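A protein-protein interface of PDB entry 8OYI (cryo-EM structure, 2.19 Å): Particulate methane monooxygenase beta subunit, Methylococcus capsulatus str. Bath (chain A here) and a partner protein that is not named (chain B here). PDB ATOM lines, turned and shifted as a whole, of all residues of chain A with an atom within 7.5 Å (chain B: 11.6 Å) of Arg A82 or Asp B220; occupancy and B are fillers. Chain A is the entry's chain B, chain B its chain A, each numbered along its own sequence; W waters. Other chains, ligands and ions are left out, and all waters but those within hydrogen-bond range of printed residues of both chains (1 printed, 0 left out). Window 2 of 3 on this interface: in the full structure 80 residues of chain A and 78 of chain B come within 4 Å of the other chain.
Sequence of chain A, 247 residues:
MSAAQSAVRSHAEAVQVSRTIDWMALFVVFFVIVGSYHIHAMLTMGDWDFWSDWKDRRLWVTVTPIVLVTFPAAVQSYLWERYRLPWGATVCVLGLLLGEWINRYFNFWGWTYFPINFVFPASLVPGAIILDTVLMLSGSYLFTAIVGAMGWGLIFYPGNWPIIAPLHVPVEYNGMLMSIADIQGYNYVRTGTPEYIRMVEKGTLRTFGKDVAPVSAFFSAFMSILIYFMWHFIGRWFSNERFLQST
Among the printed residues, pairs that only touch across the chains: Tyr A83 with Phe B212 (3.0 Å), Arg A82 with Leu B216 (3.4 Å), Arg A82 with Val B219 (3.4 Å), Tyr A83 with Leu B216 (3.5 Å), Glu A81 with Val B219 (3.5 Å), Leu A85 with Ile B211 (3.6 Å), Leu A85 with Arg B215 (3.7 Å), Arg A84 with Val B228 (3.7 Å), Trp A80 with Val B228 (3.96 Å) and Tyr A83 with Val B219 (3.98 Å).
The side-chain carboxylate (OD1) of Asp B220 lies within salt-bridge range of the guanidinium group (NH2) of Arg A82 (2.9 Å). The guanidinium group of Arg B215 is in hydrogen-bond range of the backbone carbonyl oxygen of Arg A84 (2.8 Å). The guanidinium group (NE) of Arg B215 sits at hydrogen-bond distance from the backbone carbonyl oxygen (O) of Tyr A83, at 2.7 Å.
The backbone NH (N) of Glu A81 is in hydrogen-bond range of the side-chain hydroxyl (OH) of Tyr A141 (3.1 Å). NH1 of Arg A82 lies within salt-bridge range of OE2 of Glu A241. The backbone carbonyl oxygen (O) of Glu A81 sits at hydrogen-bond distance from the guanidinium group (NH1) of Arg A84 (3.3 Å). O of Trp A80 is in hydrogen-bond range of NH1 of Arg A84, at 2.7 Å. The backbone carbonyl oxygen (O) of Leu A79 lies within hydrogen-bond range of the backbone NH (N) of Arg A84 (3.3 Å). NH2 of Arg B215 is in hydrogen-bond range of O of Leu B227 (3.3 Å).
Of the printed residues of chain B, Trp A80 touches Val B228. Glu A81 touches just one residue of chain B: Val B219 (3.5 Å). Tyr A83 touches four residues of chain B. Printed residues of chain B within 4 Å of Leu A85: Ile B211 and Arg B215. Of the printed residues of chain A, Arg B215 touches Tyr A83 (2.7 Å), Arg A84 (2.8 Å) and Leu A85 (3.7 Å). Of chain A, only Arg A82 comes within 4 Å of Asp B220.
Water W1 lies within hydrogen-bond range of the side-chain carboxylate of Asp B220, the guanidinium group of Arg A82 and the backbone carbonyl oxygen of Leu B216.
Of the 19 printed residues of chain B, 7 touch a printed residue of chain A. Among the printed residues, Asp or Glu carboxylates within 4 Å of a Lys or Arg side-chain nitrogen of the other chain: Arg A82 with Asp B220 (2.9 Å).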
ATOM      1  N   GLN A  76       0.354  23.125   2.946  1.00  0.00           N
ATOM      2  CA  GLN A  76       1.614  23.847   2.819  1.00  0.00           C
ATOM      3  C   GLN A  76       2.797  22.906   3.007  1.00  0.00           C
ATOM      4  O   GLN A  76       3.719  22.879   2.183  1.00  0.00           O
ATOM      5  CB  GLN A  76       1.664  24.978   3.840  1.00  0.00           C
ATOM      6  CG  GLN A  76       1.342  26.343   3.281  1.00  0.00           C
ATOM      7  CD  GLN A  76       1.544  27.438   4.304  1.00  0.00           C
ATOM      8  OE1 GLN A  76       1.761  27.165   5.484  1.00  0.00           O
ATOM      9  NE2 GLN A  76       1.480  28.684   3.857  1.00  0.00           N
ATOM     10  N   SER A  77       2.761  22.099   4.074  1.00  0.00           N
ATOM     11  CA  SER A  77       3.855  21.178   4.359  1.00  0.00           C
ATOM     12  C   SER A  77       4.085  20.206   3.213  1.00  0.00           C
ATOM     13  O   SER A  77       5.189  19.679   3.058  1.00  0.00           O
ATOM     14  CB  SER A  77       3.568  20.407   5.647  1.00  0.00           C
ATOM     15  OG  SER A  77       2.859  19.209   5.375  1.00  0.00           O
ATOM     16  N   TYR A  78       3.054  19.949   2.416  1.00  0.00           N
ATOM     17  CA  TYR A  78       3.249  19.092   1.248  1.00  0.00           C
ATOM     18  C   TYR A  78       3.704  19.891   0.028  1.00  0.00           C
ATOM     19  O   TYR A  78       4.739  19.587  -0.576  1.00  0.00           O
ATOM     20  CB  TYR A  78       1.965  18.330   0.937  1.00  0.00           C
ATOM     21  CG  TYR A  78       1.960  17.640  -0.406  1.00  0.00           C
ATOM     22  CD1 TYR A  78       2.734  16.510  -0.632  1.00  0.00           C
ATOM     23  CD2 TYR A  78       1.172  18.112  -1.449  1.00  0.00           C
ATOM     24  CE1 TYR A  78       2.727  15.874  -1.856  1.00  0.00           C
ATOM     25  CE2 TYR A  78       1.158  17.480  -2.674  1.00  0.00           C
ATOM     26  CZ  TYR A  78       1.938  16.361  -2.873  1.00  0.00           C
ATOM     27  OH  TYR A  78       1.929  15.732  -4.093  1.00  0.00           O
ATOM     28  N   LEU A  79       2.928  20.910  -0.351  1.00  0.00           N
ATOM     29  CA  LEU A  79       3.171  21.614  -1.604  1.00  0.00           C
ATOM     30  C   LEU A  79       4.508  22.339  -1.586  1.00  0.00           C
ATOM     31  O   LEU A  79       5.301  22.209  -2.522  1.00  0.00           O
ATOM     32  CB  LEU A  79       2.034  22.597  -1.882  1.00  0.00           C
ATOM     33  CG  LEU A  79       0.727  21.998  -2.403  1.00  0.00           C
ATOM     34  CD1 LEU A  79      -0.256  23.098  -2.761  1.00  0.00           C
ATOM     35  CD2 LEU A  79       0.985  21.096  -3.602  1.00  0.00           C
ATOM     36  N   TRP A  80       4.781  23.112  -0.532  1.00  0.00           N
ATOM     37  CA  TRP A  80       6.051  23.828  -0.478  1.00  0.00           C
ATOM     38  C   TRP A  80       7.222  22.855  -0.472  1.00  0.00           C
ATOM     39  O   TRP A  80       8.163  22.997  -1.259  1.00  0.00           O
ATOM     40  CB  TRP A  80       6.092  24.736   0.748  1.00  0.00           C
ATOM     41  CG  TRP A  80       7.383  25.470   0.888  1.00  0.00           C
ATOM     42  CD1 TRP A  80       8.343  25.268   1.836  1.00  0.00           C
ATOM     43  CD2 TRP A  80       7.876  26.508   0.034  1.00  0.00           C
ATOM     44  NE1 TRP A  80       9.396  26.125   1.636  1.00  0.00           N
ATOM     45  CE2 TRP A  80       9.133  26.897   0.535  1.00  0.00           C
ATOM     46  CE3 TRP A  80       7.373  27.151  -1.099  1.00  0.00           C
ATOM     47  CZ2 TRP A  80       9.894  27.901  -0.060  1.00  0.00           C
ATOM     48  CZ3 TRP A  80       8.129  28.145  -1.686  1.00  0.00           C
ATOM     49  CH2 TRP A  80       9.376  28.509  -1.166  1.00  0.00           C
ATOM     50  N   GLU A  81       7.146  21.821   0.368  1.00  0.00           N
ATOM     51  CA  GLU A  81       8.258  20.886   0.496  1.00  0.00           C
ATOM     52  C   GLU A  81       8.538  20.144  -0.805  1.00  0.00           C
ATOM     53  O   GLU A  81       9.704  19.911  -1.141  1.00  0.00           O
ATOM     54  CB  GLU A  81       7.979  19.890   1.621  1.00  0.00           C
ATOM     55  CG  GLU A  81       9.168  19.018   2.012  1.00  0.00           C
ATOM     56  CD  GLU A  81      10.326  19.805   2.604  1.00  0.00           C
ATOM     57  OE1 GLU A  81      10.139  20.987   2.966  1.00  0.00           O
ATOM     58  OE2 GLU A  81      11.431  19.234   2.714  1.00  0.00           O
ATOM     59  N   ARG A  82       7.498  19.763  -1.550  1.00  0.00           N
ATOM     60  CA  ARG A  82       7.701  18.900  -2.703  1.00  0.00           C
ATOM     61  C   ARG A  82       7.780  19.641  -4.033  1.00  0.00           C
ATOM     62  O   ARG A  82       8.345  19.093  -4.987  1.00  0.00           O
ATOM     63  CB  ARG A  82       6.587  17.850  -2.782  1.00  0.00           C
ATOM     64  CG  ARG A  82       6.583  16.862  -1.624  1.00  0.00           C
ATOM     65  CD  ARG A  82       7.982  16.344  -1.320  1.00  0.00           C
ATOM     66  NE  ARG A  82       8.569  15.634  -2.451  1.00  0.00           N
ATOM     67  CZ  ARG A  82       8.399  14.344  -2.694  1.00  0.00           C
ATOM     68  NH1 ARG A  82       7.667  13.582  -1.901  1.00  0.00           N
ATOM     69  NH2 ARG A  82       8.980  13.801  -3.760  1.00  0.00           N
ATOM     70  N   TYR A  83       7.242  20.858  -4.137  1.00  0.00           N
ATOM     71  CA  TYR A  83       7.227  21.564  -5.408  1.00  0.00           C
ATOM     72  C   TYR A  83       7.658  23.020  -5.301  1.00  0.00           C
ATOM     73  O   TYR A  83       7.748  23.685  -6.339  1.00  0.00           O
ATOM     74  CB  TYR A  83       5.820  21.519  -6.035  1.00  0.00           C
ATOM     75  CG  TYR A  83       5.139  20.171  -6.006  1.00  0.00           C
ATOM     76  CD1 TYR A  83       4.447  19.741  -4.882  1.00  0.00           C
ATOM     77  CD2 TYR A  83       5.168  19.335  -7.112  1.00  0.00           C
ATOM     78  CE1 TYR A  83       3.817  18.513  -4.856  1.00  0.00           C
ATOM     79  CE2 TYR A  83       4.542  18.107  -7.097  1.00  0.00           C
ATOM     80  CZ  TYR A  83       3.869  17.701  -5.967  1.00  0.00           C
ATOM     81  OH  TYR A  83       3.244  16.476  -5.948  1.00  0.00           O
ATOM     82  N   ARG A  84       7.927  23.536  -4.100  1.00  0.00           N
ATOM     83  CA  ARG A  84       8.157  24.965  -3.886  1.00  0.00           C
ATOM     84  C   ARG A  84       6.999  25.795  -4.430  1.00  0.00           C
ATOM     85  O   ARG A  84       7.191  26.844  -5.046  1.00  0.00           O
ATOM     86  CB  ARG A  84       9.489  25.409  -4.488  1.00  0.00           C
ATOM     87  CG  ARG A  84      10.697  24.819  -3.791  1.00  0.00           C
ATOM     88  CD  ARG A  84      10.942  25.507  -2.458  1.00  0.00           C
ATOM     89  NE  ARG A  84      12.019  24.886  -1.697  1.00  0.00           N
ATOM     90  CZ  ARG A  84      11.948  23.693  -1.123  1.00  0.00           C
ATOM     91  NH1 ARG A  84      10.846  22.960  -1.178  1.00  0.00           N
ATOM     92  NH2 ARG A  84      13.005  23.224  -0.468  1.00  0.00           N
ATOM     93  N   LEU A  85       5.778  25.312  -4.200  1.00  0.00           N
ATOM     94  CA  LEU A  85       4.567  26.042  -4.569  1.00  0.00           C
ATOM     95  C   LEU A  85       3.999  26.701  -3.322  1.00  0.00           C
ATOM     96  O   LEU A  85       3.433  26.013  -2.458  1.00  0.00           O
ATOM     97  CB  LEU A  85       3.534  25.098  -5.194  1.00  0.00           C
ATOM     98  CG  LEU A  85       3.812  24.640  -6.623  1.00  0.00           C
ATOM     99  CD1 LEU A  85       2.879  23.510  -7.005  1.00  0.00           C
ATOM    100  CD2 LEU A  85       3.675  25.800  -7.590  1.00  0.00           C
ATOM    101  N   TYR A 141       9.592  26.292   8.322  1.00  0.00           N
ATOM    102  CA  TYR A 141       8.258  25.907   8.769  1.00  0.00           C
ATOM    103  C   TYR A 141       8.006  26.324  10.212  1.00  0.00           C
ATOM    104  O   TYR A 141       6.875  26.673  10.560  1.00  0.00           O
ATOM    105  CB  TYR A 141       8.057  24.400   8.610  1.00  0.00           C
ATOM    106  CG  TYR A 141       7.808  23.961   7.189  1.00  0.00           C
ATOM    107  CD1 TYR A 141       6.605  24.239   6.559  1.00  0.00           C
ATOM    108  CD2 TYR A 141       8.776  23.269   6.475  1.00  0.00           C
ATOM    109  CE1 TYR A 141       6.368  23.839   5.259  1.00  0.00           C
ATOM    110  CE2 TYR A 141       8.553  22.865   5.178  1.00  0.00           C
ATOM    111  CZ  TYR A 141       7.348  23.153   4.574  1.00  0.00           C
ATOM    112  OH  TYR A 141       7.125  22.750   3.282  1.00  0.00           O
ATOM    113  N   ARG A 236       2.606  15.968   6.783  1.00  0.00           N
ATOM    114  CA  ARG A 236       3.802  15.190   6.478  1.00  0.00           C
ATOM    115  C   ARG A 236       3.477  13.705   6.412  1.00  0.00           C
ATOM    116  O   ARG A 236       3.900  13.004   5.486  1.00  0.00           O
ATOM    117  CB  ARG A 236       4.880  15.456   7.529  1.00  0.00           C
ATOM    118  CG  ARG A 236       5.774  16.635   7.214  1.00  0.00           C
ATOM    119  CD  ARG A 236       6.255  16.586   5.778  1.00  0.00           C
ATOM    120  NE  ARG A 236       6.410  17.922   5.214  1.00  0.00           N
ATOM    121  CZ  ARG A 236       7.452  18.711   5.431  1.00  0.00           C
ATOM    122  NH1 ARG A 236       8.464  18.325   6.191  1.00  0.00           N
ATOM    123  NH2 ARG A 236       7.476  19.917   4.876  1.00  0.00           N
ATOM    124  N   SER A 239       1.348  12.638   3.342  1.00  0.00           N
ATOM    125  CA  SER A 239       2.093  12.654   2.057  1.00  0.00           C
ATOM    126  C   SER A 239       2.800  11.315   1.822  1.00  0.00           C
ATOM    127  O   SER A 239       3.195  11.076   0.679  1.00  0.00           O
ATOM    128  CB  SER A 239       3.066  13.801   2.028  1.00  0.00           C
ATOM    129  OG  SER A 239       2.383  15.041   2.087  1.00  0.00           O
ATOM    130  N   ASN A 240       2.916  10.460   2.845  1.00  0.00           N
ATOM    131  CA  ASN A 240       3.649   9.163   2.740  1.00  0.00           C
ATOM    132  C   ASN A 240       3.391   8.469   1.395  1.00  0.00           C
ATOM    133  O   ASN A 240       2.221   8.393   0.975  1.00  0.00           O
ATOM    134  CB  ASN A 240       3.364   8.250   3.941  1.00  0.00           C
ATOM    135  CG  ASN A 240       2.167   7.337   3.767  1.00  0.00           C
ATOM    136  OD1 ASN A 240       2.309   6.199   3.331  1.00  0.00           O
ATOM    137  ND2 ASN A 240       0.985   7.826   4.108  1.00  0.00           N
ATOM    138  N   GLU A 241       4.451   7.990   0.738  1.00  0.00           N
ATOM    139  CA  GLU A 241       4.309   7.249  -0.512  1.00  0.00           C
ATOM    140  C   GLU A 241       4.562   5.765  -0.291  1.00  0.00           C
ATOM    141  O   GLU A 241       5.063   5.063  -1.175  1.00  0.00           O
ATOM    142  CB  GLU A 241       5.254   7.795  -1.577  1.00  0.00           C
ATOM    143  CG  GLU A 241       5.100   9.277  -1.850  1.00  0.00           C
ATOM    144  CD  GLU A 241       6.431   9.972  -2.047  1.00  0.00           C
ATOM    145  OE1 GLU A 241       7.317   9.393  -2.709  1.00  0.00           O
ATOM    146  OE2 GLU A 241       6.596  11.099  -1.535  1.00  0.00           O
ATOM    147  N   PRO B 210       5.038  26.063 -15.328  1.00  0.00           N
ATOM    148  CA  PRO B 210       4.638  24.676 -15.066  1.00  0.00           C
ATOM    149  C   PRO B 210       4.557  24.394 -13.573  1.00  0.00           C
ATOM    150  O   PRO B 210       5.331  24.927 -12.776  1.00  0.00           O
ATOM    151  CB  PRO B 210       5.740  23.853 -15.745  1.00  0.00           C
ATOM    152  CG  PRO B 210       6.837  24.829 -16.067  1.00  0.00           C
ATOM    153  CD  PRO B 210       6.148  26.128 -16.293  1.00  0.00           C
ATOM    154  N   ILE B 211       3.600  23.542 -13.194  1.00  0.00           N
ATOM    155  CA  ILE B 211       3.168  23.468 -11.802  1.00  0.00           C
ATOM    156  C   ILE B 211       3.706  22.248 -11.065  1.00  0.00           C
ATOM    157  O   ILE B 211       4.438  22.387 -10.082  1.00  0.00           O
ATOM    158  CB  ILE B 211       1.632  23.502 -11.719  1.00  0.00           C
ATOM    159  CG1 ILE B 211       1.085  24.746 -12.418  1.00  0.00           C
ATOM    160  CG2 ILE B 211       1.175  23.459 -10.269  1.00  0.00           C
ATOM    161  CD1 ILE B 211      -0.394  24.671 -12.712  1.00  0.00           C
ATOM    162  N   PHE B 212       3.334  21.041 -11.499  1.00  0.00           N
ATOM    163  CA  PHE B 212       3.484  19.882 -10.624  1.00  0.00           C
ATOM    164  C   PHE B 212       4.699  19.013 -10.932  1.00  0.00           C
ATOM    165  O   PHE B 212       5.596  18.890 -10.094  1.00  0.00           O
ATOM    166  CB  PHE B 212       2.206  19.034 -10.683  1.00  0.00           C
ATOM    167  CG  PHE B 212       1.069  19.607  -9.894  1.00  0.00           C
ATOM    168  CD1 PHE B 212       1.154  19.718  -8.518  1.00  0.00           C
ATOM    169  CD2 PHE B 212      -0.082  20.036 -10.528  1.00  0.00           C
ATOM    170  CE1 PHE B 212       0.110  20.247  -7.788  1.00  0.00           C
ATOM    171  CE2 PHE B 212      -1.129  20.568  -9.803  1.00  0.00           C
ATOM    172  CZ  PHE B 212      -1.034  20.674  -8.432  1.00  0.00           C
ATOM    173  N   ILE B 213       4.770  18.430 -12.122  1.00  0.00           N
ATOM    174  CA  ILE B 213       5.736  17.356 -12.347  1.00  0.00           C
ATOM    175  C   ILE B 213       7.142  17.912 -12.560  1.00  0.00           C
ATOM    176  O   ILE B 213       8.088  17.400 -11.942  1.00  0.00           O
ATOM    177  CB  ILE B 213       5.306  16.448 -13.512  1.00  0.00           C
ATOM    178  CG1 ILE B 213       4.050  15.660 -13.133  1.00  0.00           C
ATOM    179  CG2 ILE B 213       6.418  15.477 -13.848  1.00  0.00           C
ATOM    180  CD1 ILE B 213       3.782  14.465 -14.021  1.00  0.00           C
ATOM    181  N   PRO B 214       7.356  18.913 -13.425  1.00  0.00           N
ATOM    182  CA  PRO B 214       8.715  19.474 -13.524  1.00  0.00           C
ATOM    183  C   PRO B 214       9.221  20.067 -12.222  1.00  0.00           C
ATOM    184  O   PRO B 214      10.403  19.910 -11.899  1.00  0.00           O
ATOM    185  CB  PRO B 214       8.577  20.538 -14.624  1.00  0.00           C
ATOM    186  CG  PRO B 214       7.132  20.828 -14.705  1.00  0.00           C
ATOM    187  CD  PRO B 214       6.447  19.547 -14.397  1.00  0.00           C
ATOM    188  N   ARG B 215       8.356  20.724 -11.445  1.00  0.00           N
ATOM    189  CA  ARG B 215       8.796  21.267 -10.160  1.00  0.00           C
ATOM    190  C   ARG B 215       9.134  20.152  -9.181  1.00  0.00           C
ATOM    191  O   ARG B 215      10.113  20.250  -8.434  1.00  0.00           O
ATOM    192  CB  ARG B 215       7.730  22.196  -9.578  1.00  0.00           C
ATOM    193  CG  ARG B 215       7.606  23.526 -10.301  1.00  0.00           C
ATOM    194  CD  ARG B 215       6.608  24.447  -9.627  1.00  0.00           C
ATOM    195  NE  ARG B 215       7.206  25.209  -8.539  1.00  0.00           N
ATOM    196  CZ  ARG B 215       7.727  26.420  -8.672  1.00  0.00           C
ATOM    197  NH1 ARG B 215       7.757  27.034  -9.843  1.00  0.00           N
ATOM    198  NH2 ARG B 215       8.230  27.031  -7.604  1.00  0.00           N
ATOM    199  N   LEU B 216       8.336  19.081  -9.175  1.00  0.00           N
ATOM    200  CA  LEU B 216       8.638  17.933  -8.327  1.00  0.00           C
ATOM    201  C   LEU B 216       9.983  17.318  -8.699  1.00  0.00           C
ATOM    202  O   LEU B 216      10.787  16.988  -7.819  1.00  0.00           O
ATOM    203  CB  LEU B 216       7.526  16.894  -8.451  1.00  0.00           C
ATOM    204  CG  LEU B 216       7.749  15.522  -7.818  1.00  0.00           C
ATOM    205  CD1 LEU B 216       7.703  15.620  -6.304  1.00  0.00           C
ATOM    206  CD2 LEU B 216       6.720  14.525  -8.327  1.00  0.00           C
ATOM    207  N   LEU B 217      10.237  17.163 -10.000  1.00  0.00           N
ATOM    208  CA  LEU B 217      11.507  16.600 -10.444  1.00  0.00           C
ATOM    209  C   LEU B 217      12.675  17.511 -10.085  1.00  0.00           C
ATOM    210  O   LEU B 217      13.743  17.031  -9.694  1.00  0.00           O
ATOM    211  CB  LEU B 217      11.470  16.346 -11.952  1.00  0.00           C
ATOM    212  CG  LEU B 217      10.573  15.201 -12.419  1.00  0.00           C
ATOM    213  CD1 LEU B 217      10.492  15.172 -13.936  1.00  0.00           C
ATOM    214  CD2 LEU B 217      11.068  13.873 -11.881  1.00  0.00           C
ATOM    215  N   MET B 218      12.494  18.825 -10.221  1.00  0.00           N
ATOM    216  CA  MET B 218      13.555  19.758  -9.854  1.00  0.00           C
ATOM    217  C   MET B 218      13.854  19.698  -8.362  1.00  0.00           C
ATOM    218  O   MET B 218      15.021  19.733  -7.958  1.00  0.00           O
ATOM    219  CB  MET B 218      13.172  21.179 -10.265  1.00  0.00           C
ATOM    220  CG  MET B 218      13.289  21.441 -11.756  1.00  0.00           C
ATOM    221  SD  MET B 218      14.992  21.698 -12.272  1.00  0.00           S
ATOM    222  CE  MET B 218      15.363  23.239 -11.439  1.00  0.00           C
ATOM    223  N   VAL B 219      12.814  19.616  -7.530  1.00  0.00           N
ATOM    224  CA  VAL B 219      13.028  19.544  -6.088  1.00  0.00           C
ATOM    225  C   VAL B 219      13.705  18.231  -5.707  1.00  0.00           C
ATOM    226  O   VAL B 219      14.620  18.209  -4.875  1.00  0.00           O
ATOM    227  CB  VAL B 219      11.699  19.737  -5.336  1.00  0.00           C
ATOM    228  CG1 VAL B 219      11.876  19.440  -3.857  1.00  0.00           C
ATOM    229  CG2 VAL B 219      11.182  21.153  -5.531  1.00  0.00           C
ATOM    230  N   ASP B 220      13.278  17.119  -6.314  1.00  0.00           N
ATOM    231  CA  ASP B 220      13.842  15.815  -5.968  1.00  0.00           C
ATOM    232  C   ASP B 220      15.288  15.688  -6.443  1.00  0.00           C
ATOM    233  O   ASP B 220      16.202  15.449  -5.647  1.00  0.00           O
ATOM    234  CB  ASP B 220      12.980  14.696  -6.559  1.00  0.00           C
ATOM    235  CG  ASP B 220      11.654  14.542  -5.840  1.00  0.00           C
ATOM    236  OD1 ASP B 220      11.621  14.712  -4.603  1.00  0.00           O
ATOM    237  OD2 ASP B 220      10.645  14.245  -6.511  1.00  0.00           O
ATOM    238  N   ALA B 221      15.511  15.845  -7.747  1.00  0.00           N
ATOM    239  CA  ALA B 221      16.841  15.674  -8.318  1.00  0.00           C
ATOM    240  C   ALA B 221      17.717  16.877  -8.005  1.00  0.00           C
ATOM    241  O   ALA B 221      17.711  17.868  -8.740  1.00  0.00           O
ATOM    242  CB  ALA B 221      16.754  15.456  -9.828  1.00  0.00           C
ATOM    243  N   GLY B 222      18.473  16.795  -6.913  1.00  0.00           N
ATOM    244  CA  GLY B 222      19.336  17.880  -6.503  1.00  0.00           C
ATOM    245  C   GLY B 222      18.578  18.981  -5.790  1.00  0.00           C
ATOM    246  O   GLY B 222      17.356  18.955  -5.639  1.00  0.00           O
ATOM    247  N   ARG B 223      19.340  19.973  -5.339  1.00  0.00           N
ATOM    248  CA  ARG B 223      18.743  21.140  -4.708  1.00  0.00           C
ATOM    249  C   ARG B 223      17.955  21.934  -5.744  1.00  0.00           C
ATOM    250  O   ARG B 223      18.365  22.071  -6.900  1.00  0.00           O
ATOM    251  CB  ARG B 223      19.828  22.016  -4.087  1.00  0.00           C
ATOM    252  CG  ARG B 223      20.379  21.486  -2.777  1.00  0.00           C
ATOM    253  CD  ARG B 223      21.558  22.322  -2.310  1.00  0.00           C
ATOM    254  NE  ARG B 223      22.079  21.867  -1.028  1.00  0.00           N
ATOM    255  CZ  ARG B 223      23.366  21.861  -0.704  1.00  0.00           C
ATOM    256  NH1 ARG B 223      24.290  22.289  -1.548  1.00  0.00           N
ATOM    257  NH2 ARG B 223      23.732  21.411   0.490  1.00  0.00           N
ATOM    258  N   ALA B 224      16.804  22.460  -5.327  1.00  0.00           N
ATOM    259  CA  ALA B 224      15.983  23.156  -6.306  1.00  0.00           C
ATOM    260  C   ALA B 224      16.466  24.584  -6.505  1.00  0.00           C
ATOM    261  O   ALA B 224      17.067  24.893  -7.538  1.00  0.00           O
ATOM    262  CB  ALA B 224      14.518  23.155  -5.865  1.00  0.00           C
ATOM    263  N   ASP B 225      16.233  25.440  -5.508  1.00  0.00           N
ATOM    264  CA  ASP B 225      16.822  26.782  -5.402  1.00  0.00           C
ATOM    265  C   ASP B 225      16.815  27.537  -6.732  1.00  0.00           C
ATOM    266  O   ASP B 225      17.642  28.416  -6.982  1.00  0.00           O
ATOM    267  CB  ASP B 225      18.236  26.702  -4.833  1.00  0.00           C
ATOM    268  CG  ASP B 225      18.250  26.352  -3.357  1.00  0.00           C
ATOM    269  OD1 ASP B 225      17.263  26.672  -2.664  1.00  0.00           O
ATOM    270  OD2 ASP B 225      19.245  25.761  -2.896  1.00  0.00           O
ATOM    271  N   GLU B 226      15.866  27.189  -7.600  1.00  0.00           N
ATOM    272  CA  GLU B 226      15.823  27.792  -8.925  1.00  0.00           C
ATOM    273  C   GLU B 226      14.404  28.171  -9.318  1.00  0.00           C
ATOM    274  O   GLU B 226      14.197  29.050 -10.161  1.00  0.00           O
ATOM    275  CB  GLU B 226      16.427  26.843  -9.960  1.00  0.00           C
ATOM    276  CG  GLU B 226      17.942  26.919 -10.053  1.00  0.00           C
ATOM    277  CD  GLU B 226      18.581  25.567 -10.308  1.00  0.00           C
ATOM    278  OE1 GLU B 226      18.243  24.933 -11.328  1.00  0.00           O
ATOM    279  OE2 GLU B 226      19.421  25.141  -9.488  1.00  0.00           O
ATOM    280  N   LEU B 227      13.418  27.507  -8.717  1.00  0.00           N
ATOM    281  CA  LEU B 227      12.027  27.780  -9.033  1.00  0.00           C
ATOM    282  C   LEU B 227      11.437  28.897  -8.185  1.00  0.00           C
ATOM    283  O   LEU B 227      10.329  29.360  -8.478  1.00  0.00           O
ATOM    284  CB  LEU B 227      11.194  26.506  -8.879  1.00  0.00           C
ATOM    285  CG  LEU B 227      11.852  25.265  -9.490  1.00  0.00           C
ATOM    286  CD1 LEU B 227      12.386  24.356  -8.400  1.00  0.00           C
ATOM    287  CD2 LEU B 227      10.915  24.517 -10.415  1.00  0.00           C
ATOM    288  N   VAL B 228      12.145  29.329  -7.147  1.00  0.00           N
ATOM    289  CA  VAL B 228      11.745  30.493  -6.366  1.00  0.00           C
ATOM    290  C   VAL B 228      12.917  31.463  -6.327  1.00  0.00           C
ATOM    291  O   VAL B 228      13.826  31.332  -5.500  1.00  0.00           O
ATOM    292  CB  VAL B 228      11.297  30.097  -4.947  1.00  0.00           C
ATOM    293  CG1 VAL B 228      11.018  31.335  -4.106  1.00  0.00           C
ATOM    294  CG2 VAL B 228      10.069  29.201  -5.008  1.00  0.00           C
HETATM  295  O   HOH W   1      10.193  16.836  -4.437  1.00  0.00           O
